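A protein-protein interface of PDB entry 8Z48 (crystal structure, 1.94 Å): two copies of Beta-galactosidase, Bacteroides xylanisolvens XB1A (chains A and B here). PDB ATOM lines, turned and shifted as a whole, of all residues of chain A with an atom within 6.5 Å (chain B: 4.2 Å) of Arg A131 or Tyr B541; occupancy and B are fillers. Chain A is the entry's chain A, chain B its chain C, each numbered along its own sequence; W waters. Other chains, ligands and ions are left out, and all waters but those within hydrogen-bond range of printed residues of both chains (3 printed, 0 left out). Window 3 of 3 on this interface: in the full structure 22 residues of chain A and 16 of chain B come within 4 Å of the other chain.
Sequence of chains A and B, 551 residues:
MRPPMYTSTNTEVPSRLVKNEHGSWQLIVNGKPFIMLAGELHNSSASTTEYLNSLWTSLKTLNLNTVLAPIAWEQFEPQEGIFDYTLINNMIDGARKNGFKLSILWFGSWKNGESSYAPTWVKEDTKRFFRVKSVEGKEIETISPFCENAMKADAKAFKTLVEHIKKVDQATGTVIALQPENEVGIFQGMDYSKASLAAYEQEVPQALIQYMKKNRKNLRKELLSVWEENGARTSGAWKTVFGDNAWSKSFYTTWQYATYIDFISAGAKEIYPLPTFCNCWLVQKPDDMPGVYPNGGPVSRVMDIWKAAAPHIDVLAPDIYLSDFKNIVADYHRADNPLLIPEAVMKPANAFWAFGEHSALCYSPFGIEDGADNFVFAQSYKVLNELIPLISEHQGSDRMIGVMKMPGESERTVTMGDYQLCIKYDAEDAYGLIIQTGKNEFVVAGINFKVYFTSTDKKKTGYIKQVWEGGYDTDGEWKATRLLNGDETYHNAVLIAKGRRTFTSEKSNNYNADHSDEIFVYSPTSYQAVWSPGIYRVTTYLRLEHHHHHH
The side-chain carboxylate (OE2) of Glu A141 sits at hydrogen-bond distance from the side-chain hydroxyl (OH) of Tyr B541, 2.6 Å away.
O of Glu A139 sits at hydrogen-bond distance from NH1 of Arg B543 (3.0 Å).
OE2 of Glu A124 lies within salt-bridge range of NZ of Lys B465, 3.0 Å away.
The side-chain carboxylate (OE1) of Glu A141 lies within salt-bridge range of the guanidinium group (NH2) of Arg B543.
The guanidinium group (NE) of Arg B543 sits close to the guanidinium group (NH1) of Arg A131, 3.3 Å away.
NH2 of Arg A131 lies within hydrogen-bond range of OH of Tyr B541 (2.9 Å).
The side-chain amino group (NZ) of Lys A123 lies within hydrogen-bond range of the backbone carbonyl oxygen (O) of Lys B465, at 2.7 Å.
O of Glu A141 lies within hydrogen-bond range of N of Ser A115.
The backbone carbonyl oxygen of Tyr B463 is in hydrogen-bond range of the backbone NH of Tyr B541 (2.9 Å).
The backbone NH (N) of Arg B543 sits at hydrogen-bond distance from the backbone carbonyl oxygen (O) of Thr B461, at 3.0 Å.
The guanidinium group (NH1) of Arg A131 lies within salt-bridge range of the side-chain carboxylate (OE1) of Glu A141 (3.0 Å).
OH of Tyr B419 lies close to N of Tyr B541, 3.4 Å away.
The backbone carbonyl oxygen (O) of Lys A123 lies within hydrogen-bond range of the guanidinium group (NH2) of Arg A131.
Printed residues of chain B that touch a printed residue of chain A: Tyr B463, Lys B465, Tyr B541 and Arg B543.
Hydrophobic or aromatic side chains of chain B that line the printed part of chain A: Tyr B463 and Tyr B541.
Of the 21 printed residues of chain A, 7 touch a printed residue of chain B.
Among the printed residues, 11 pairs touch across the chains.
Thr A120 touches Lys B465.
Lys A123 touches Tyr B541 (CB to OH, 3.8 Å).
Ile A140 touches Arg B543 (C to NH2, 3.8 Å).
Tyr B463 touches Glu A141.
No position is printed for both chains.
Of chain B, only Tyr B541 and Arg B543 come within 4 Å of Arg A131.
Of the printed residues of chain B, Glu A139 touches Arg B543.
Of the printed residues of chain A, Tyr B463 touches Glu A141 (3.6 Å).
Of the printed residues of chain A, Tyr B541 touches Lys A123 (3.8 Å), Arg A131 (2.9 Å) and Glu A141 (2.6 Å).
Printed residues of chain A within 4 Å of Arg B543: Arg A131 (3.3 Å), Glu A139 (3.0 Å), Ile A140 (3.8 Å) and Glu A141 (2.8 Å).
The nearest printed residue of chain B that does not touch Ile A140 is Tyr B463 (6.6 Å).
Water W1 lies within hydrogen-bond range of the side-chain amino group (NZ) of Lys B465, the backbone carbonyl oxygen (O) of Thr B540 and the side-chain carboxylate (OE2) of Glu A124.
Water W2 lies within hydrogen-bond range of the backbone carbonyl oxygen (O) of Ile B464, the side-chain carboxylate (OE2) of Glu A141 and the side-chain amino group (NZ) of Lys A123.
Water W3 bridges the backbone carbonyl oxygen of Lys B465 (3.0 Å) and the side-chain amino group of Lys A123 (3.3 Å).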
ATOM      1  N   SER A 115      21.962  30.364 -31.938  1.00  0.00           N
ATOM      2  CA  SER A 115      21.116  29.179 -31.853  1.00  0.00           C
ATOM      3  C   SER A 115      20.119  29.229 -30.692  1.00  0.00           C
ATOM      4  O   SER A 115      19.805  28.190 -30.095  1.00  0.00           O
ATOM      5  CB  SER A 115      21.989  27.934 -31.792  1.00  0.00           C
ATOM      6  OG  SER A 115      22.814  27.902 -32.954  1.00  0.00           O
ATOM      7  N   THR A 120      15.564  22.703 -26.366  1.00  0.00           N
ATOM      8  CA  THR A 120      16.314  22.451 -25.149  1.00  0.00           C
ATOM      9  C   THR A 120      17.224  21.231 -25.325  1.00  0.00           C
ATOM     10  O   THR A 120      18.362  21.250 -24.870  1.00  0.00           O
ATOM     11  CB  THR A 120      15.355  22.280 -23.967  1.00  0.00           C
ATOM     12  OG1 THR A 120      14.423  21.258 -24.277  1.00  0.00           O
ATOM     13  CG2 THR A 120      14.560  23.543 -23.670  1.00  0.00           C
ATOM     14  N   VAL A 122      18.515  20.011 -28.034  1.00  0.00           N
ATOM     15  CA  VAL A 122      19.628  20.337 -28.906  1.00  0.00           C
ATOM     16  C   VAL A 122      20.669  21.150 -28.127  1.00  0.00           C
ATOM     17  O   VAL A 122      21.874  20.837 -28.156  1.00  0.00           O
ATOM     18  CB  VAL A 122      19.155  21.064 -30.177  1.00  0.00           C
ATOM     19  CG1 VAL A 122      20.344  21.533 -31.015  1.00  0.00           C
ATOM     20  CG2 VAL A 122      18.218  20.185 -31.015  1.00  0.00           C
ATOM     21  N   LYS A 123      20.207  22.178 -27.403  1.00  0.00           N
ATOM     22  CA  LYS A 123      21.109  23.035 -26.654  1.00  0.00           C
ATOM     23  C   LYS A 123      21.924  22.218 -25.639  1.00  0.00           C
ATOM     24  O   LYS A 123      23.131  22.424 -25.482  1.00  0.00           O
ATOM     25  CB  LYS A 123      20.290  24.116 -25.931  1.00  0.00           C
ATOM     26  CG  LYS A 123      19.679  25.185 -26.834  1.00  0.00           C
ATOM     27  CD  LYS A 123      18.886  26.218 -26.052  1.00  0.00           C
ATOM     28  CE  LYS A 123      18.281  27.261 -26.936  1.00  0.00           C
ATOM     29  NZ  LYS A 123      17.348  28.077 -26.177  1.00  0.00           N
ATOM     30  N   GLU A 124      21.257  21.303 -24.936  1.00  0.00           N
ATOM     31  CA  GLU A 124      21.830  20.685 -23.750  1.00  0.00           C
ATOM     32  C   GLU A 124      22.846  19.601 -24.097  1.00  0.00           C
ATOM     33  O   GLU A 124      23.562  19.146 -23.207  1.00  0.00           O
ATOM     34  CB  GLU A 124      20.735  20.102 -22.859  1.00  0.00           C
ATOM     35  CG  GLU A 124      19.967  21.171 -22.098  1.00  0.00           C
ATOM     36  CD  GLU A 124      18.994  20.602 -21.079  1.00  0.00           C
ATOM     37  OE1 GLU A 124      18.293  19.618 -21.411  1.00  0.00           O
ATOM     38  OE2 GLU A 124      18.928  21.163 -19.965  1.00  0.00           O
ATOM     39  N   ASP A 125      22.883  19.178 -25.366  1.00  0.00           N
ATOM     40  CA  ASP A 125      23.818  18.164 -25.821  1.00  0.00           C
ATOM     41  C   ASP A 125      24.850  18.770 -26.775  1.00  0.00           C
ATOM     42  O   ASP A 125      24.730  18.600 -27.991  1.00  0.00           O
ATOM     43  CB  ASP A 125      23.095  16.982 -26.454  1.00  0.00           C
ATOM     44  CG  ASP A 125      23.993  15.796 -26.784  1.00  0.00           C
ATOM     45  OD1 ASP A 125      25.240  15.943 -26.695  1.00  0.00           O
ATOM     46  OD2 ASP A 125      23.445  14.765 -27.180  1.00  0.00           O
ATOM     47  N   THR A 126      25.915  19.358 -26.208  1.00  0.00           N
ATOM     48  CA  THR A 126      26.972  19.979 -26.993  1.00  0.00           C
ATOM     49  C   THR A 126      27.978  18.951 -27.531  1.00  0.00           C
ATOM     50  O   THR A 126      28.866  19.322 -28.297  1.00  0.00           O
ATOM     51  CB  THR A 126      27.667  21.074 -26.177  1.00  0.00           C
ATOM     52  OG1 THR A 126      28.227  20.524 -24.993  1.00  0.00           O
ATOM     53  CG2 THR A 126      26.715  22.187 -25.786  1.00  0.00           C
ATOM     54  N   PHE A 129      25.576  18.043 -30.711  1.00  0.00           N
ATOM     55  CA  PHE A 129      25.413  19.249 -31.513  1.00  0.00           C
ATOM     56  C   PHE A 129      26.466  20.258 -31.083  1.00  0.00           C
ATOM     57  O   PHE A 129      26.208  21.137 -30.258  1.00  0.00           O
ATOM     58  CB  PHE A 129      23.986  19.765 -31.348  1.00  0.00           C
ATOM     59  CG  PHE A 129      22.903  18.740 -31.631  1.00  0.00           C
ATOM     60  CD1 PHE A 129      22.666  18.294 -32.922  1.00  0.00           C
ATOM     61  CD2 PHE A 129      22.096  18.258 -30.605  1.00  0.00           C
ATOM     62  CE1 PHE A 129      21.651  17.395 -33.177  1.00  0.00           C
ATOM     63  CE2 PHE A 129      21.104  17.319 -30.859  1.00  0.00           C
ATOM     64  CZ  PHE A 129      20.875  16.900 -32.144  1.00  0.00           C
ATOM     65  N   PHE A 130      27.675  20.122 -31.615  1.00  0.00           N
ATOM     66  CA  PHE A 130      28.792  20.911 -31.119  1.00  0.00           C
ATOM     67  C   PHE A 130      28.640  22.363 -31.562  1.00  0.00           C
ATOM     68  O   PHE A 130      28.021  22.668 -32.588  1.00  0.00           O
ATOM     69  CB  PHE A 130      30.166  20.325 -31.461  1.00  0.00           C
ATOM     70  CG  PHE A 130      30.485  20.102 -32.931  1.00  0.00           C
ATOM     71  CD1 PHE A 130      30.997  21.135 -33.722  1.00  0.00           C
ATOM     72  CD2 PHE A 130      30.303  18.858 -33.521  1.00  0.00           C
ATOM     73  CE1 PHE A 130      31.273  20.932 -35.062  1.00  0.00           C
ATOM     74  CE2 PHE A 130      30.612  18.659 -34.862  1.00  0.00           C
ATOM     75  CZ  PHE A 130      31.082  19.693 -35.627  1.00  0.00           C
ATOM     76  N   ARG A 131      29.199  23.245 -30.722  1.00  0.00           N
ATOM     77  CA  ARG A 131      29.082  24.680 -30.860  1.00  0.00           C
ATOM     78  C   ARG A 131      30.241  25.239 -31.669  1.00  0.00           C
ATOM     79  O   ARG A 131      31.286  24.610 -31.826  1.00  0.00           O
ATOM     80  CB  ARG A 131      29.144  25.350 -29.482  1.00  0.00           C
ATOM     81  CG  ARG A 131      28.088  24.859 -28.505  1.00  0.00           C
ATOM     82  CD  ARG A 131      26.683  24.926 -29.092  1.00  0.00           C
ATOM     83  NE  ARG A 131      25.609  24.663 -28.130  1.00  0.00           N
ATOM     84  CZ  ARG A 131      25.295  25.428 -27.099  1.00  0.00           C
ATOM     85  NH1 ARG A 131      25.920  26.573 -26.888  1.00  0.00           N
ATOM     86  NH2 ARG A 131      24.345  25.036 -26.283  1.00  0.00           N
ATOM     87  N   VAL A 132      30.024  26.456 -32.166  1.00  0.00           N
ATOM     88  CA  VAL A 132      31.094  27.297 -32.673  1.00  0.00           C
ATOM     89  C   VAL A 132      32.036  27.644 -31.522  1.00  0.00           C
ATOM     90  O   VAL A 132      31.576  27.918 -30.399  1.00  0.00           O
ATOM     91  CB  VAL A 132      30.528  28.575 -33.312  1.00  0.00           C
ATOM     92  CG1 VAL A 132      31.631  29.573 -33.657  1.00  0.00           C
ATOM     93  CG2 VAL A 132      29.681  28.271 -34.544  1.00  0.00           C
ATOM     94  N   LYS A 133      33.338  27.706 -31.838  1.00  0.00           N
ATOM     95  CA  LYS A 133      34.349  28.122 -30.871  1.00  0.00           C
ATOM     96  C   LYS A 133      34.997  29.410 -31.352  1.00  0.00           C
ATOM     97  O   LYS A 133      35.235  29.559 -32.552  1.00  0.00           O
ATOM     98  CB  LYS A 133      35.438  27.068 -30.659  1.00  0.00           C
ATOM     99  CG  LYS A 133      34.932  25.875 -29.891  1.00  0.00           C
ATOM    100  CD  LYS A 133      35.956  24.758 -29.764  1.00  0.00           C
ATOM    101  CE  LYS A 133      35.397  23.618 -28.977  1.00  0.00           C
ATOM    102  NZ  LYS A 133      36.494  22.779 -28.496  1.00  0.00           N
ATOM    103  N   GLU A 139      33.278  28.140 -26.263  1.00  0.00           N
ATOM    104  CA  GLU A 139      32.094  27.659 -26.951  1.00  0.00           C
ATOM    105  C   GLU A 139      30.961  28.667 -26.785  1.00  0.00           C
ATOM    106  O   GLU A 139      30.568  28.949 -25.647  1.00  0.00           O
ATOM    107  CB  GLU A 139      31.587  26.356 -26.331  1.00  0.00           C
ATOM    108  CG  GLU A 139      32.276  25.115 -26.885  1.00  0.00           C
ATOM    109  CD  GLU A 139      32.005  23.848 -26.106  1.00  0.00           C
ATOM    110  OE1 GLU A 139      30.848  23.368 -26.078  1.00  0.00           O
ATOM    111  OE2 GLU A 139      32.993  23.325 -25.557  1.00  0.00           O
ATOM    112  N   ILE A 140      30.360  29.109 -27.905  1.00  0.00           N
ATOM    113  CA  ILE A 140      29.335  30.155 -27.858  1.00  0.00           C
ATOM    114  C   ILE A 140      27.946  29.528 -28.014  1.00  0.00           C
ATOM    115  O   ILE A 140      27.822  28.359 -28.331  1.00  0.00           O
ATOM    116  CB  ILE A 140      29.602  31.267 -28.891  1.00  0.00           C
ATOM    117  CG1 ILE A 140      29.624  30.758 -30.336  1.00  0.00           C
ATOM    118  CG2 ILE A 140      30.893  32.008 -28.540  1.00  0.00           C
ATOM    119  CD1 ILE A 140      29.578  31.867 -31.385  1.00  0.00           C
ATOM    120  N   GLU A 141      26.899  30.345 -27.829  1.00  0.00           N
ATOM    121  CA  GLU A 141      25.524  29.907 -27.993  1.00  0.00           C
ATOM    122  C   GLU A 141      25.137  29.869 -29.474  1.00  0.00           C
ATOM    123  O   GLU A 141      24.098  30.412 -29.853  1.00  0.00           O
ATOM    124  CB  GLU A 141      24.620  30.838 -27.184  1.00  0.00           C
ATOM    125  CG  GLU A 141      23.270  30.216 -26.852  1.00  0.00           C
ATOM    126  CD  GLU A 141      23.332  29.095 -25.822  1.00  0.00           C
ATOM    127  OE1 GLU A 141      24.451  28.708 -25.375  1.00  0.00           O
ATOM    128  OE2 GLU A 141      22.219  28.639 -25.460  1.00  0.00           O
ATOM    129  N   THR A 142      26.011  29.282 -30.310  1.00  0.00           N
ATOM    130  CA  THR A 142      25.768  29.066 -31.726  1.00  0.00           C
ATOM    131  C   THR A 142      26.209  27.639 -32.059  1.00  0.00           C
ATOM    132  O   THR A 142      27.351  27.280 -31.780  1.00  0.00           O
ATOM    133  CB  THR A 142      26.552  30.056 -32.581  1.00  0.00           C
ATOM    134  OG1 THR A 142      26.206  31.393 -32.274  1.00  0.00           O
ATOM    135  CG2 THR A 142      26.336  29.843 -34.075  1.00  0.00           C
ATOM    136  N   ILE A 143      25.312  26.853 -32.678  1.00  0.00           N
ATOM    137  CA  ILE A 143      25.623  25.525 -33.190  1.00  0.00           C
ATOM    138  C   ILE A 143      26.555  25.696 -34.392  1.00  0.00           C
ATOM    139  O   ILE A 143      26.313  26.551 -35.240  1.00  0.00           O
ATOM    140  CB  ILE A 143      24.321  24.788 -33.594  1.00  0.00           C
ATOM    141  CG1 ILE A 143      23.373  24.612 -32.429  1.00  0.00           C
ATOM    142  CG2 ILE A 143      24.615  23.463 -34.298  1.00  0.00           C
ATOM    143  CD1 ILE A 143      21.991  24.130 -32.835  1.00  0.00           C
ATOM    144  N   SER A 144      27.580  24.838 -34.512  1.00  0.00           N
ATOM    145  CA  SER A 144      28.548  24.964 -35.595  1.00  0.00           C
ATOM    146  C   SER A 144      27.933  24.562 -36.933  1.00  0.00           C
ATOM    147  O   SER A 144      27.312  23.500 -37.044  1.00  0.00           O
ATOM    148  CB  SER A 144      29.794  24.125 -35.330  1.00  0.00           C
ATOM    149  OG  SER A 144      30.656  24.142 -36.470  1.00  0.00           O
ATOM    150  N   CYS A 147      28.657  20.917 -37.997  1.00  0.00           N
ATOM    151  CA  CYS A 147      28.017  19.803 -37.298  1.00  0.00           C
ATOM    152  C   CYS A 147      26.892  19.131 -38.101  1.00  0.00           C
ATOM    153  O   CYS A 147      25.782  19.638 -38.132  1.00  0.00           O
ATOM    154  CB  CYS A 147      27.472  20.290 -35.961  1.00  0.00           C
ATOM    155  SG  CYS A 147      26.659  18.989 -34.992  1.00  0.00           S
ATOM    156  N   ASP A 191      35.023  29.840 -37.640  1.00  0.00           N
ATOM    157  CA  ASP A 191      34.781  28.946 -36.516  1.00  0.00           C
ATOM    158  C   ASP A 191      36.086  28.216 -36.184  1.00  0.00           C
ATOM    159  O   ASP A 191      36.761  27.757 -37.101  1.00  0.00           O
ATOM    160  CB  ASP A 191      33.668  27.965 -36.856  1.00  0.00           C
ATOM    161  CG  ASP A 191      33.341  26.891 -35.831  1.00  0.00           C
ATOM    162  OD1 ASP A 191      33.782  27.037 -34.675  1.00  0.00           O
ATOM    163  OD2 ASP A 191      32.640  25.916 -36.223  1.00  0.00           O
ATOM    164  N   SER A 193      36.228  25.573 -34.087  1.00  0.00           N
ATOM    165  CA  SER A 193      35.952  24.191 -33.756  1.00  0.00           C
ATOM    166  C   SER A 193      36.903  23.321 -34.560  1.00  0.00           C
ATOM    167  O   SER A 193      37.349  23.738 -35.626  1.00  0.00           O
ATOM    168  CB  SER A 193      34.520  23.814 -34.027  1.00  0.00           C
ATOM    169  OG  SER A 193      34.217  23.848 -35.419  1.00  0.00           O
ATOM    170  N   TYR B 419      23.863  29.955  -9.939  1.00  0.00           N
ATOM    171  CA  TYR B 419      24.013  31.069 -10.859  1.00  0.00           C
ATOM    172  C   TYR B 419      24.316  32.371 -10.136  1.00  0.00           C
ATOM    173  O   TYR B 419      24.018  32.536  -8.946  1.00  0.00           O
ATOM    174  CB  TYR B 419      22.754  31.240 -11.709  1.00  0.00           C
ATOM    175  CG  TYR B 419      22.438  30.002 -12.530  1.00  0.00           C
ATOM    176  CD1 TYR B 419      22.950  29.821 -13.808  1.00  0.00           C
ATOM    177  CD2 TYR B 419      21.617  29.007 -12.006  1.00  0.00           C
ATOM    178  CE1 TYR B 419      22.683  28.668 -14.540  1.00  0.00           C
ATOM    179  CE2 TYR B 419      21.324  27.867 -12.732  1.00  0.00           C
ATOM    180  CZ  TYR B 419      21.856  27.698 -14.006  1.00  0.00           C
ATOM    181  OH  TYR B 419      21.503  26.573 -14.693  1.00  0.00           O
ATOM    182  N   THR B 461      29.755  27.108 -18.136  1.00  0.00           N
ATOM    183  CA  THR B 461      29.085  28.265 -18.708  1.00  0.00           C
ATOM    184  C   THR B 461      27.599  28.133 -18.407  1.00  0.00           C
ATOM    185  O   THR B 461      26.971  27.130 -18.733  1.00  0.00           O
ATOM    186  CB  THR B 461      29.349  28.429 -20.206  1.00  0.00           C
ATOM    187  OG1 THR B 461      30.741  28.695 -20.290  1.00  0.00           O
ATOM    188  CG2 THR B 461      28.700  29.666 -20.807  1.00  0.00           C
ATOM    189  N   GLY B 462      27.072  29.147 -17.724  1.00  0.00           N
ATOM    190  CA  GLY B 462      25.645  29.252 -17.466  1.00  0.00           C
ATOM    191  C   GLY B 462      24.972  30.192 -18.465  1.00  0.00           C
ATOM    192  O   GLY B 462      25.535  31.213 -18.856  1.00  0.00           O
ATOM    193  N   TYR B 463      23.738  29.855 -18.844  1.00  0.00           N
ATOM    194  CA  TYR B 463      23.035  30.635 -19.839  1.00  0.00           C
ATOM    195  C   TYR B 463      21.534  30.508 -19.630  1.00  0.00           C
ATOM    196  O   TYR B 463      21.059  29.492 -19.112  1.00  0.00           O
ATOM    197  CB  TYR B 463      23.380  30.074 -21.222  1.00  0.00           C
ATOM    198  CG  TYR B 463      23.614  31.167 -22.242  1.00  0.00           C
ATOM    199  CD1 TYR B 463      24.811  31.869 -22.234  1.00  0.00           C
ATOM    200  CD2 TYR B 463      22.671  31.508 -23.191  1.00  0.00           C
ATOM    201  CE1 TYR B 463      25.052  32.891 -23.129  1.00  0.00           C
ATOM    202  CE2 TYR B 463      22.917  32.507 -24.118  1.00  0.00           C
ATOM    203  CZ  TYR B 463      24.112  33.203 -24.087  1.00  0.00           C
ATOM    204  OH  TYR B 463      24.428  34.229 -24.945  1.00  0.00           O
ATOM    205  N   ILE B 464      20.791  31.497 -20.129  1.00  0.00           N
ATOM    206  CA  ILE B 464      19.346  31.377 -20.214  1.00  0.00           C
ATOM    207  C   ILE B 464      19.006  30.241 -21.160  1.00  0.00           C
ATOM    208  O   ILE B 464      19.600  30.134 -22.242  1.00  0.00           O
ATOM    209  CB  ILE B 464      18.695  32.693 -20.678  1.00  0.00           C
ATOM    210  CG1 ILE B 464      18.781  33.750 -19.570  1.00  0.00           C
ATOM    211  CG2 ILE B 464      17.262  32.464 -21.171  1.00  0.00           C
ATOM    212  CD1 ILE B 464      18.530  35.174 -20.030  1.00  0.00           C
ATOM    213  N   LYS B 465      18.016  29.430 -20.769  1.00  0.00           N
ATOM    214  CA  LYS B 465      17.584  28.328 -21.615  1.00  0.00           C
ATOM    215  C   LYS B 465      16.371  28.754 -22.439  1.00  0.00           C
ATOM    216  O   LYS B 465      16.428  28.721 -23.674  1.00  0.00           O
ATOM    217  CB  LYS B 465      17.310  27.036 -20.832  1.00  0.00           C
ATOM    218  CG  LYS B 465      17.271  25.813 -21.747  1.00  0.00           C
ATOM    219  CD  LYS B 465      16.610  24.567 -21.167  1.00  0.00           C
ATOM    220  CE  LYS B 465      16.786  24.351 -19.707  1.00  0.00           C
ATOM    221  NZ  LYS B 465      16.634  22.933 -19.367  1.00  0.00           N
ATOM    222  N   THR B 540      17.217  28.293 -16.955  1.00  0.00           N
ATOM    223  CA  THR B 540      18.639  28.420 -17.204  1.00  0.00           C
ATOM    224  C   THR B 540      19.230  27.024 -17.380  1.00  0.00           C
ATOM    225  O   THR B 540      18.576  26.024 -17.098  1.00  0.00           O
ATOM    226  CB  THR B 540      19.324  29.112 -16.018  1.00  0.00           C
ATOM    227  OG1 THR B 540      18.991  28.363 -14.839  1.00  0.00           O
ATOM    228  CG2 THR B 540      18.932  30.575 -15.858  1.00  0.00           C
ATOM    229  N   TYR B 541      20.455  26.956 -17.892  1.00  0.00           N
ATOM    230  CA  TYR B 541      21.193  25.699 -17.912  1.00  0.00           C
ATOM    231  C   TYR B 541      22.686  25.976 -17.775  1.00  0.00           C
ATOM    232  O   TYR B 541      23.136  27.084 -18.080  1.00  0.00           O
ATOM    233  CB  TYR B 541      20.831  24.922 -19.178  1.00  0.00           C
ATOM    234  CG  TYR B 541      21.420  25.395 -20.509  1.00  0.00           C
ATOM    235  CD1 TYR B 541      21.135  26.648 -21.046  1.00  0.00           C
ATOM    236  CD2 TYR B 541      22.107  24.503 -21.321  1.00  0.00           C
ATOM    237  CE1 TYR B 541      21.614  27.034 -22.291  1.00  0.00           C
ATOM    238  CE2 TYR B 541      22.567  24.865 -22.576  1.00  0.00           C
ATOM    239  CZ  TYR B 541      22.323  26.135 -23.068  1.00  0.00           C
ATOM    240  OH  TYR B 541      22.820  26.440 -24.317  1.00  0.00           O
ATOM    241  N   LEU B 542      23.419  24.939 -17.342  1.00  0.00           N
ATOM    242  CA  LEU B 542      24.879  24.912 -17.304  1.00  0.00           C
ATOM    243  C   LEU B 542      25.375  23.912 -18.357  1.00  0.00           C
ATOM    244  O   LEU B 542      24.746  22.881 -18.548  1.00  0.00           O
ATOM    245  CB  LEU B 542      25.344  24.486 -15.911  1.00  0.00           C
ATOM    246  CG  LEU B 542      24.823  25.296 -14.720  1.00  0.00           C
ATOM    247  CD1 LEU B 542      24.919  24.477 -13.438  1.00  0.00           C
ATOM    248  CD2 LEU B 542      25.580  26.597 -14.576  1.00  0.00           C
ATOM    249  N   ARG B 543      26.489  24.224 -19.036  1.00  0.00           N
ATOM    250  CA  ARG B 543      27.112  23.310 -19.991  1.00  0.00           C
ATOM    251  C   ARG B 543      28.635  23.291 -19.769  1.00  0.00           C
ATOM    252  O   ARG B 543      29.111  24.127 -18.955  1.00  0.00           O
ATOM    253  CB  ARG B 543      26.780  23.683 -21.444  1.00  0.00           C
ATOM    254  CG  ARG B 543      27.178  25.076 -21.919  1.00  0.00           C
ATOM    255  CD  ARG B 543      26.529  25.412 -23.264  1.00  0.00           C
ATOM    256  NE  ARG B 543      26.398  26.838 -23.592  1.00  0.00           N
ATOM    257  CZ  ARG B 543      27.377  27.627 -24.044  1.00  0.00           C
ATOM    258  NH1 ARG B 543      28.618  27.178 -24.133  1.00  0.00           N
ATOM    259  NH2 ARG B 543      27.114  28.874 -24.411  1.00  0.00           N
HETATM  260  O   HOH W   1      18.255  23.210 -17.378  1.00  0.00           O
HETATM  261  O   HOH W   2      19.579  29.614 -24.991  1.00  0.00           O
HETATM  262  O   HOH W   3      14.681  29.903 -25.816  1.00  0.00           O
